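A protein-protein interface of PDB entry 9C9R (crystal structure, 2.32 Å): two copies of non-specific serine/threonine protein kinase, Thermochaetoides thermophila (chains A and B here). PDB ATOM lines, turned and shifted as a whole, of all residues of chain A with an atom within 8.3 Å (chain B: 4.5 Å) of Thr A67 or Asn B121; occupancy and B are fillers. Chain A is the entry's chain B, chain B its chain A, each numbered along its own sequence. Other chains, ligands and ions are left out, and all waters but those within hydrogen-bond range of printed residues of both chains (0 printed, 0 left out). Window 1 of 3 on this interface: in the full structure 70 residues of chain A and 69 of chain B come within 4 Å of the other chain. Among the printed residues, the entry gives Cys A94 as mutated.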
ATOM      1  N   PRO A  64     -22.252 -24.176 -18.188  1.00  0.00           N
ATOM      2  CA  PRO A  64     -22.882 -23.374 -17.140  1.00  0.00           C
ATOM      3  C   PRO A  64     -22.700 -24.031 -15.786  1.00  0.00           C
ATOM      4  O   PRO A  64     -22.441 -25.226 -15.678  1.00  0.00           O
ATOM      5  CB  PRO A  64     -24.360 -23.366 -17.539  1.00  0.00           C
ATOM      6  CG  PRO A  64     -24.544 -24.715 -18.198  1.00  0.00           C
ATOM      7  CD  PRO A  64     -23.241 -24.985 -18.932  1.00  0.00           C
ATOM      8  N   THR A  65     -22.846 -23.227 -14.745  1.00  0.00           N
ATOM      9  CA  THR A  65     -22.755 -23.710 -13.377  1.00  0.00           C
ATOM     10  C   THR A  65     -24.040 -23.406 -12.621  1.00  0.00           C
ATOM     11  O   THR A  65     -24.703 -22.392 -12.865  1.00  0.00           O
ATOM     12  CB  THR A  65     -21.572 -23.074 -12.639  1.00  0.00           C
ATOM     13  OG1 THR A  65     -21.781 -21.660 -12.520  1.00  0.00           O
ATOM     14  CG2 THR A  65     -20.271 -23.344 -13.406  1.00  0.00           C
ATOM     15  N   ALA A  66     -24.378 -24.292 -11.693  1.00  0.00           N
ATOM     16  CA  ALA A  66     -25.541 -24.092 -10.847  1.00  0.00           C
ATOM     17  C   ALA A  66     -25.345 -22.879  -9.947  1.00  0.00           C
ATOM     18  O   ALA A  66     -24.243 -22.601  -9.479  1.00  0.00           O
ATOM     19  CB  ALA A  66     -25.795 -25.339 -10.002  1.00  0.00           C
ATOM     20  N   THR A  67     -26.426 -22.144  -9.714  1.00  0.00           N
ATOM     21  CA  THR A  67     -26.385 -20.985  -8.828  1.00  0.00           C
ATOM     22  C   THR A  67     -26.645 -21.352  -7.367  1.00  0.00           C
ATOM     23  O   THR A  67     -26.049 -20.744  -6.475  1.00  0.00           O
ATOM     24  CB  THR A  67     -27.395 -19.946  -9.330  1.00  0.00           C
ATOM     25  OG1 THR A  67     -27.015 -19.546 -10.654  1.00  0.00           O
ATOM     26  CG2 THR A  67     -27.475 -18.721  -8.418  1.00  0.00           C
ATOM     27  N   LEU A  68     -27.481 -22.356  -7.099  1.00  0.00           N
ATOM     28  CA  LEU A  68     -27.783 -22.749  -5.733  1.00  0.00           C
ATOM     29  C   LEU A  68     -28.410 -24.134  -5.755  1.00  0.00           C
ATOM     30  O   LEU A  68     -28.928 -24.578  -6.783  1.00  0.00           O
ATOM     31  CB  LEU A  68     -28.710 -21.738  -5.031  1.00  0.00           C
ATOM     32  CG  LEU A  68     -30.216 -21.745  -5.329  1.00  0.00           C
ATOM     33  CD1 LEU A  68     -30.913 -20.721  -4.458  1.00  0.00           C
ATOM     34  CD2 LEU A  68     -30.505 -21.473  -6.800  1.00  0.00           C
ATOM     35  N   TYR A  69     -28.359 -24.803  -4.605  1.00  0.00           N
ATOM     36  CA  TYR A  69     -28.802 -26.188  -4.478  1.00  0.00           C
ATOM     37  C   TYR A  69     -28.942 -26.514  -2.984  1.00  0.00           C
ATOM     38  O   TYR A  69     -28.445 -25.766  -2.143  1.00  0.00           O
ATOM     39  CB  TYR A  69     -27.813 -27.150  -5.166  1.00  0.00           C
ATOM     40  CG  TYR A  69     -26.355 -26.778  -4.992  1.00  0.00           C
ATOM     41  CD1 TYR A  69     -25.672 -27.087  -3.819  1.00  0.00           C
ATOM     42  CD2 TYR A  69     -25.658 -26.130  -6.009  1.00  0.00           C
ATOM     43  CE1 TYR A  69     -24.337 -26.752  -3.651  1.00  0.00           C
ATOM     44  CE2 TYR A  69     -24.321 -25.788  -5.860  1.00  0.00           C
ATOM     45  CZ  TYR A  69     -23.663 -26.108  -4.677  1.00  0.00           C
ATOM     46  OH  TYR A  69     -22.335 -25.770  -4.527  1.00  0.00           O
ATOM     47  N   VAL A  80     -22.885 -19.856   2.776  1.00  0.00           N
ATOM     48  CA  VAL A  80     -24.105 -19.058   2.779  1.00  0.00           C
ATOM     49  C   VAL A  80     -25.302 -19.998   2.683  1.00  0.00           C
ATOM     50  O   VAL A  80     -25.424 -20.778   1.730  1.00  0.00           O
ATOM     51  CB  VAL A  80     -24.112 -18.043   1.631  1.00  0.00           C
ATOM     52  CG1 VAL A  80     -25.340 -17.142   1.732  1.00  0.00           C
ATOM     53  CG2 VAL A  80     -22.838 -17.227   1.652  1.00  0.00           C
ATOM     54  N   LEU A  82     -29.553 -20.424   2.715  1.00  0.00           N
ATOM     55  CA  LEU A  82     -30.791 -19.719   2.400  1.00  0.00           C
ATOM     56  C   LEU A  82     -31.960 -20.706   2.392  1.00  0.00           C
ATOM     57  O   LEU A  82     -31.800 -21.886   2.064  1.00  0.00           O
ATOM     58  CB  LEU A  82     -30.703 -18.999   1.042  1.00  0.00           C
ATOM     59  CG  LEU A  82     -29.522 -18.070   0.753  1.00  0.00           C
ATOM     60  CD1 LEU A  82     -29.416 -17.747  -0.752  1.00  0.00           C
ATOM     61  CD2 LEU A  82     -29.654 -16.785   1.569  1.00  0.00           C
ATOM     62  N   LEU A  90     -30.943 -24.288   1.267  1.00  0.00           N
ATOM     63  CA  LEU A  90     -30.114 -24.227   0.068  1.00  0.00           C
ATOM     64  C   LEU A  90     -28.807 -23.505   0.386  1.00  0.00           C
ATOM     65  O   LEU A  90     -28.721 -22.743   1.357  1.00  0.00           O
ATOM     66  CB  LEU A  90     -30.844 -23.481  -1.070  1.00  0.00           C
ATOM     67  CG  LEU A  90     -32.305 -23.863  -1.363  1.00  0.00           C
ATOM     68  CD1 LEU A  90     -33.013 -22.850  -2.259  1.00  0.00           C
ATOM     69  CD2 LEU A  90     -32.398 -25.276  -1.959  1.00  0.00           C
ATOM     70  N   GLN A  91     -27.785 -23.704  -0.458  1.00  0.00           N
ATOM     71  CA  GLN A  91     -26.579 -22.896  -0.321  1.00  0.00           C
ATOM     72  C   GLN A  91     -26.179 -22.222  -1.629  1.00  0.00           C
ATOM     73  O   GLN A  91     -26.491 -22.694  -2.724  1.00  0.00           O
ATOM     74  CB  GLN A  91     -25.413 -23.707   0.192  1.00  0.00           C
ATOM     75  CG  GLN A  91     -24.968 -24.815  -0.716  1.00  0.00           C
ATOM     76  CD  GLN A  91     -23.778 -25.565  -0.139  1.00  0.00           C
ATOM     77  OE1 GLN A  91     -23.941 -26.608   0.500  1.00  0.00           O
ATOM     78  NE2 GLN A  91     -22.577 -25.018  -0.334  1.00  0.00           N
ATOM     79  N   LEU A  92     -25.507 -21.075  -1.488  1.00  0.00           N
ATOM     80  CA  LEU A  92     -24.657 -20.593  -2.554  1.00  0.00           C
ATOM     81  C   LEU A  92     -23.380 -21.432  -2.577  1.00  0.00           C
ATOM     82  O   LEU A  92     -22.988 -22.009  -1.550  1.00  0.00           O
ATOM     83  CB  LEU A  92     -24.324 -19.114  -2.355  1.00  0.00           C
ATOM     84  CG  LEU A  92     -25.540 -18.177  -2.278  1.00  0.00           C
ATOM     85  CD1 LEU A  92     -25.112 -16.709  -2.308  1.00  0.00           C
ATOM     86  CD2 LEU A  92     -26.532 -18.486  -3.404  1.00  0.00           C
ATOM     87  N   PRO A  93     -22.735 -21.556  -3.743  1.00  0.00           N
ATOM     88  CA  PRO A  93     -21.565 -22.440  -3.839  1.00  0.00           C
ATOM     89  C   PRO A  93     -20.409 -21.932  -2.986  1.00  0.00           C
ATOM     90  O   PRO A  93     -20.204 -20.727  -2.839  1.00  0.00           O
ATOM     91  CB  PRO A  93     -21.214 -22.405  -5.332  1.00  0.00           C
ATOM     92  CG  PRO A  93     -22.447 -21.952  -6.028  1.00  0.00           C
ATOM     93  CD  PRO A  93     -23.177 -21.063  -5.065  1.00  0.00           C
ATOM     94  N   CYS A  94     -19.672 -22.870  -2.396  1.00  0.00           N
ATOM     95  CA  CYS A  94     -18.338 -22.624  -1.861  1.00  0.00           C
ATOM     96  C   CYS A  94     -17.231 -23.048  -2.830  1.00  0.00           C
ATOM     97  O   CYS A  94     -16.057 -22.783  -2.566  1.00  0.00           O
ATOM     98  CB  CYS A  94     -18.148 -23.369  -0.527  1.00  0.00           C
ATOM     99  SG  CYS A  94     -19.267 -22.870   0.767  1.00  0.00           S
ATOM    100  N   LEU A  96     -16.891 -24.796  -7.272  1.00  0.00           N
ATOM    101  CA  LEU A  96     -17.674 -25.217  -8.428  1.00  0.00           C
ATOM    102  C   LEU A  96     -17.806 -26.730  -8.549  1.00  0.00           C
ATOM    103  O   LEU A  96     -18.711 -27.205  -9.241  1.00  0.00           O
ATOM    104  CB  LEU A  96     -17.082 -24.636  -9.707  1.00  0.00           C
ATOM    105  CG  LEU A  96     -17.058 -23.111  -9.630  1.00  0.00           C
ATOM    106  CD1 LEU A  96     -16.419 -22.463 -10.860  1.00  0.00           C
ATOM    107  CD2 LEU A  96     -18.465 -22.584  -9.397  1.00  0.00           C
ATOM    108  N   GLY A  99     -21.478 -28.293  -7.169  1.00  0.00           N
ATOM    109  CA  GLY A  99     -22.586 -28.161  -8.105  1.00  0.00           C
ATOM    110  C   GLY A  99     -22.399 -28.974  -9.373  1.00  0.00           C
ATOM    111  O   GLY A  99     -23.357 -29.551  -9.899  1.00  0.00           O
ATOM    112  N   PHE A 119     -16.682 -20.510 -15.446  1.00  0.00           N
ATOM    113  CA  PHE A 119     -16.448 -19.406 -14.532  1.00  0.00           C
ATOM    114  C   PHE A 119     -17.678 -19.244 -13.651  1.00  0.00           C
ATOM    115  O   PHE A 119     -18.812 -19.408 -14.113  1.00  0.00           O
ATOM    116  CB  PHE A 119     -16.176 -18.103 -15.288  1.00  0.00           C
ATOM    117  CG  PHE A 119     -14.902 -18.103 -16.076  1.00  0.00           C
ATOM    118  CD1 PHE A 119     -14.869 -18.585 -17.374  1.00  0.00           C
ATOM    119  CD2 PHE A 119     -13.733 -17.591 -15.522  1.00  0.00           C
ATOM    120  CE1 PHE A 119     -13.687 -18.578 -18.090  1.00  0.00           C
ATOM    121  CE2 PHE A 119     -12.560 -17.563 -16.243  1.00  0.00           C
ATOM    122  CZ  PHE A 119     -12.531 -18.066 -17.521  1.00  0.00           C
ATOM    123  N   GLY A 120     -17.457 -18.920 -12.387  1.00  0.00           N
ATOM    124  CA  GLY A 120     -18.541 -18.944 -11.427  1.00  0.00           C
ATOM    125  C   GLY A 120     -18.151 -18.210 -10.169  1.00  0.00           C
ATOM    126  O   GLY A 120     -16.972 -17.948  -9.913  1.00  0.00           O
ATOM    127  N   ASN A 121     -19.159 -17.852  -9.393  1.00  0.00           N
ATOM    128  CA  ASN A 121     -18.935 -17.145  -8.149  1.00  0.00           C
ATOM    129  C   ASN A 121     -18.940 -18.142  -7.001  1.00  0.00           C
ATOM    130  O   ASN A 121     -19.649 -19.151  -7.040  1.00  0.00           O
ATOM    131  CB  ASN A 121     -20.007 -16.063  -7.950  1.00  0.00           C
ATOM    132  CG  ASN A 121     -19.867 -14.906  -8.958  1.00  0.00           C
ATOM    133  OD1 ASN A 121     -18.770 -14.406  -9.188  1.00  0.00           O
ATOM    134  ND2 ASN A 121     -20.976 -14.500  -9.566  1.00  0.00           N
ATOM    135  N   PHE A 123     -18.941 -18.032  -2.498  1.00  0.00           N
ATOM    136  CA  PHE A 123     -19.475 -17.122  -1.499  1.00  0.00           C
ATOM    137  C   PHE A 123     -19.048 -17.522  -0.092  1.00  0.00           C
ATOM    138  O   PHE A 123     -19.198 -18.680   0.305  1.00  0.00           O
ATOM    139  CB  PHE A 123     -21.009 -17.085  -1.605  1.00  0.00           C
ATOM    140  CG  PHE A 123     -21.504 -16.548  -2.918  1.00  0.00           C
ATOM    141  CD1 PHE A 123     -21.704 -17.401  -4.005  1.00  0.00           C
ATOM    142  CD2 PHE A 123     -21.734 -15.190  -3.081  1.00  0.00           C
ATOM    143  CE1 PHE A 123     -22.150 -16.915  -5.217  1.00  0.00           C
ATOM    144  CE2 PHE A 123     -22.183 -14.690  -4.291  1.00  0.00           C
ATOM    145  CZ  PHE A 123     -22.386 -15.558  -5.363  1.00  0.00           C
ATOM    146  N   THR B  67     -25.557 -11.280  -7.496  1.00  0.00           N
ATOM    147  CA  THR B  67     -26.234 -12.577  -7.497  1.00  0.00           C
ATOM    148  C   THR B  67     -27.594 -12.524  -6.792  1.00  0.00           C
ATOM    149  O   THR B  67     -28.519 -13.256  -7.172  1.00  0.00           O
ATOM    150  CB  THR B  67     -25.336 -13.628  -6.831  1.00  0.00           C
ATOM    151  OG1 THR B  67     -24.036 -13.597  -7.435  1.00  0.00           O
ATOM    152  CG2 THR B  67     -25.930 -15.031  -6.961  1.00  0.00           C
ATOM    153  N   PRO B  93     -32.192 -12.458  -9.317  1.00  0.00           N
ATOM    154  CA  PRO B  93     -32.577 -11.445 -10.327  1.00  0.00           C
ATOM    155  C   PRO B  93     -33.679 -11.931 -11.264  1.00  0.00           C
ATOM    156  O   PRO B  93     -33.656 -13.061 -11.746  1.00  0.00           O
ATOM    157  CB  PRO B  93     -31.272 -11.186 -11.102  1.00  0.00           C
ATOM    158  CG  PRO B  93     -30.164 -11.652 -10.193  1.00  0.00           C
ATOM    159  CD  PRO B  93     -30.761 -12.808  -9.401  1.00  0.00           C
ATOM    160  N   LEU B  96     -31.444  -7.865 -15.243  1.00  0.00           N
ATOM    161  CA  LEU B  96     -30.163  -7.368 -14.768  1.00  0.00           C
ATOM    162  C   LEU B  96     -30.203  -5.908 -14.357  1.00  0.00           C
ATOM    163  O   LEU B  96     -29.346  -5.482 -13.579  1.00  0.00           O
ATOM    164  CB  LEU B  96     -29.083  -7.582 -15.824  1.00  0.00           C
ATOM    165  CG  LEU B  96     -28.909  -9.059 -16.169  1.00  0.00           C
ATOM    166  CD1 LEU B  96     -27.878  -9.281 -17.287  1.00  0.00           C
ATOM    167  CD2 LEU B  96     -28.545  -9.839 -14.925  1.00  0.00           C
ATOM    168  N   GLY B 120     -25.449 -12.283 -17.215  1.00  0.00           N
ATOM    169  CA  GLY B 120     -25.953 -12.731 -15.937  1.00  0.00           C
ATOM    170  C   GLY B 120     -27.090 -13.696 -16.157  1.00  0.00           C
ATOM    171  O   GLY B 120     -27.574 -13.882 -17.278  1.00  0.00           O
ATOM    172  N   ASN B 121     -27.512 -14.305 -15.058  1.00  0.00           N
ATOM    173  CA  ASN B 121     -28.638 -15.217 -15.041  1.00  0.00           C
ATOM    174  C   ASN B 121     -29.859 -14.517 -14.467  1.00  0.00           C
ATOM    175  O   ASN B 121     -29.747 -13.651 -13.598  1.00  0.00           O
ATOM    176  CB  ASN B 121     -28.319 -16.460 -14.209  1.00  0.00           C
ATOM    177  CG  ASN B 121     -27.196 -17.291 -14.801  1.00  0.00           C
ATOM    178  OD1 ASN B 121     -27.170 -17.546 -16.003  1.00  0.00           O
ATOM    179  ND2 ASN B 121     -26.267 -17.719 -13.954  1.00  0.00           N
ATOM    180  N   ILE B 122     -31.026 -14.889 -14.971  1.00  0.00           N
ATOM    181  CA  ILE B 122     -32.292 -14.426 -14.420  1.00  0.00           C
ATOM    182  C   ILE B 122     -33.178 -15.644 -14.205  1.00  0.00           C
ATOM    183  O   ILE B 122     -33.016 -16.675 -14.871  1.00  0.00           O
ATOM    184  CB  ILE B 122     -32.969 -13.377 -15.322  1.00  0.00           C
ATOM    185  CG1 ILE B 122     -33.453 -14.014 -16.622  1.00  0.00           C
ATOM    186  CG2 ILE B 122     -31.994 -12.245 -15.619  1.00  0.00           C
ATOM    187  CD1 ILE B 122     -34.343 -13.096 -17.444  1.00  0.00           C
ATOM    188  N   PHE B 123     -34.104 -15.536 -13.253  1.00  0.00           N
ATOM    189  CA  PHE B 123     -34.732 -16.731 -12.687  1.00  0.00           C
ATOM    190  C   PHE B 123     -36.240 -16.562 -12.562  1.00  0.00           C
ATOM    191  O   PHE B 123     -36.711 -15.531 -12.087  1.00  0.00           O
ATOM    192  CB  PHE B 123     -34.143 -17.052 -11.311  1.00  0.00           C
ATOM    193  CG  PHE B 123     -32.674 -17.347 -11.332  1.00  0.00           C
ATOM    194  CD1 PHE B 123     -31.743 -16.313 -11.264  1.00  0.00           C
ATOM    195  CD2 PHE B 123     -32.213 -18.658 -11.391  1.00  0.00           C
ATOM    196  CE1 PHE B 123     -30.379 -16.585 -11.265  1.00  0.00           C
ATOM    197  CE2 PHE B 123     -30.860 -18.936 -11.392  1.00  0.00           C
ATOM    198  CZ  PHE B 123     -29.936 -17.896 -11.332  1.00  0.00           C
ATOM    199  N   VAL B 134     -33.768 -21.029 -15.266  1.00  0.00           N
ATOM    200  CA  VAL B 134     -32.735 -20.024 -15.490  1.00  0.00           C
ATOM    201  C   VAL B 134     -32.761 -19.609 -16.954  1.00  0.00           C
ATOM    202  O   VAL B 134     -33.124 -20.397 -17.830  1.00  0.00           O
ATOM    203  CB  VAL B 134     -31.337 -20.555 -15.116  1.00  0.00           C
ATOM    204  CG1 VAL B 134     -30.360 -19.405 -14.916  1.00  0.00           C
ATOM    205  CG2 VAL B 134     -31.426 -21.400 -13.876  1.00  0.00           C
ATOM    206  N   TYR B 135     -32.379 -18.354 -17.215  1.00  0.00           N
ATOM    207  CA  TYR B 135     -32.178 -17.829 -18.560  1.00  0.00           C
ATOM    208  C   TYR B 135     -30.996 -16.878 -18.554  1.00  0.00           C
ATOM    209  O   TYR B 135     -30.742 -16.169 -17.579  1.00  0.00           O
ATOM    210  CB  TYR B 135     -33.421 -17.078 -19.092  1.00  0.00           C
ATOM    211  CG  TYR B 135     -34.706 -17.853 -18.916  1.00  0.00           C
ATOM    212  CD1 TYR B 135     -34.979 -18.984 -19.696  1.00  0.00           C
ATOM    213  CD2 TYR B 135     -35.647 -17.462 -17.967  1.00  0.00           C
ATOM    214  CE1 TYR B 135     -36.156 -19.707 -19.528  1.00  0.00           C
ATOM    215  CE2 TYR B 135     -36.824 -18.177 -17.794  1.00  0.00           C
ATOM    216  CZ  TYR B 135     -37.074 -19.301 -18.576  1.00  0.00           C
ATOM    217  OH  TYR B 135     -38.249 -20.002 -18.403  1.00  0.00           O
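Among the printed residues, merely in contact across the chains: Phe A123 with Thr B67 (3.3 Å), Thr A67 with Phe B123 (3.4 Å), Asn A121 with Thr B67 (3.8 Å) and Thr A67 with Asn B121 (3.8 Å).
Of chain B, only Asn B121 (3.8 Å) and Phe B123 (3.4 Å) come within 4 Å of Thr A67. Asn B121 touches just one residue of chain A: Thr A67. Gly B120 touches none of the printed residues of chain A. Printed residues of chain B within 4 Å of Asn A121: Thr B67 (3.8 Å). Of the printed residues of chain B, Phe A123 touches Thr B67 (3.3 Å). Of the printed residues of chain A, Thr B67 touches Asn A121 and Phe A123. Of the printed residues of chain A, Phe B123 touches Thr A67 (3.4 Å). Tyr B135 touches none of the printed residues of chain A. Leu A82 touches none of the printed residues of chain B.
The backbone carbonyl oxygen (O) of Pro B93 lies within hydrogen-bond range of the backbone NH (N) of Phe B123. O of Pro A93 sits at hydrogen-bond distance from N of Phe A123.
Of the 9 printed residues of chain B, 3 touch a printed residue of chain A. Hydrophobic or aromatic side chains of chain B within 4 Å of the printed part of chain A: Phe B123. Of the 19 printed residues of chain A, 3 touch a printed residue of chain B. Among the printed residues, no Asp or Glu carboxylate lies within 4 Å of a Lys or Arg side-chain nitrogen of the other chain.
Thr A67 touches Asn B121, and with the chains exchanged Asn A121 touches Thr B67. Thr A67 touches Phe B123, and with the chains exchanged Phe A123 touches Thr B67. Of the 4 pairs that touch across the chains among the printed residues, 4 have their exchanged pair printed and touching as well.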
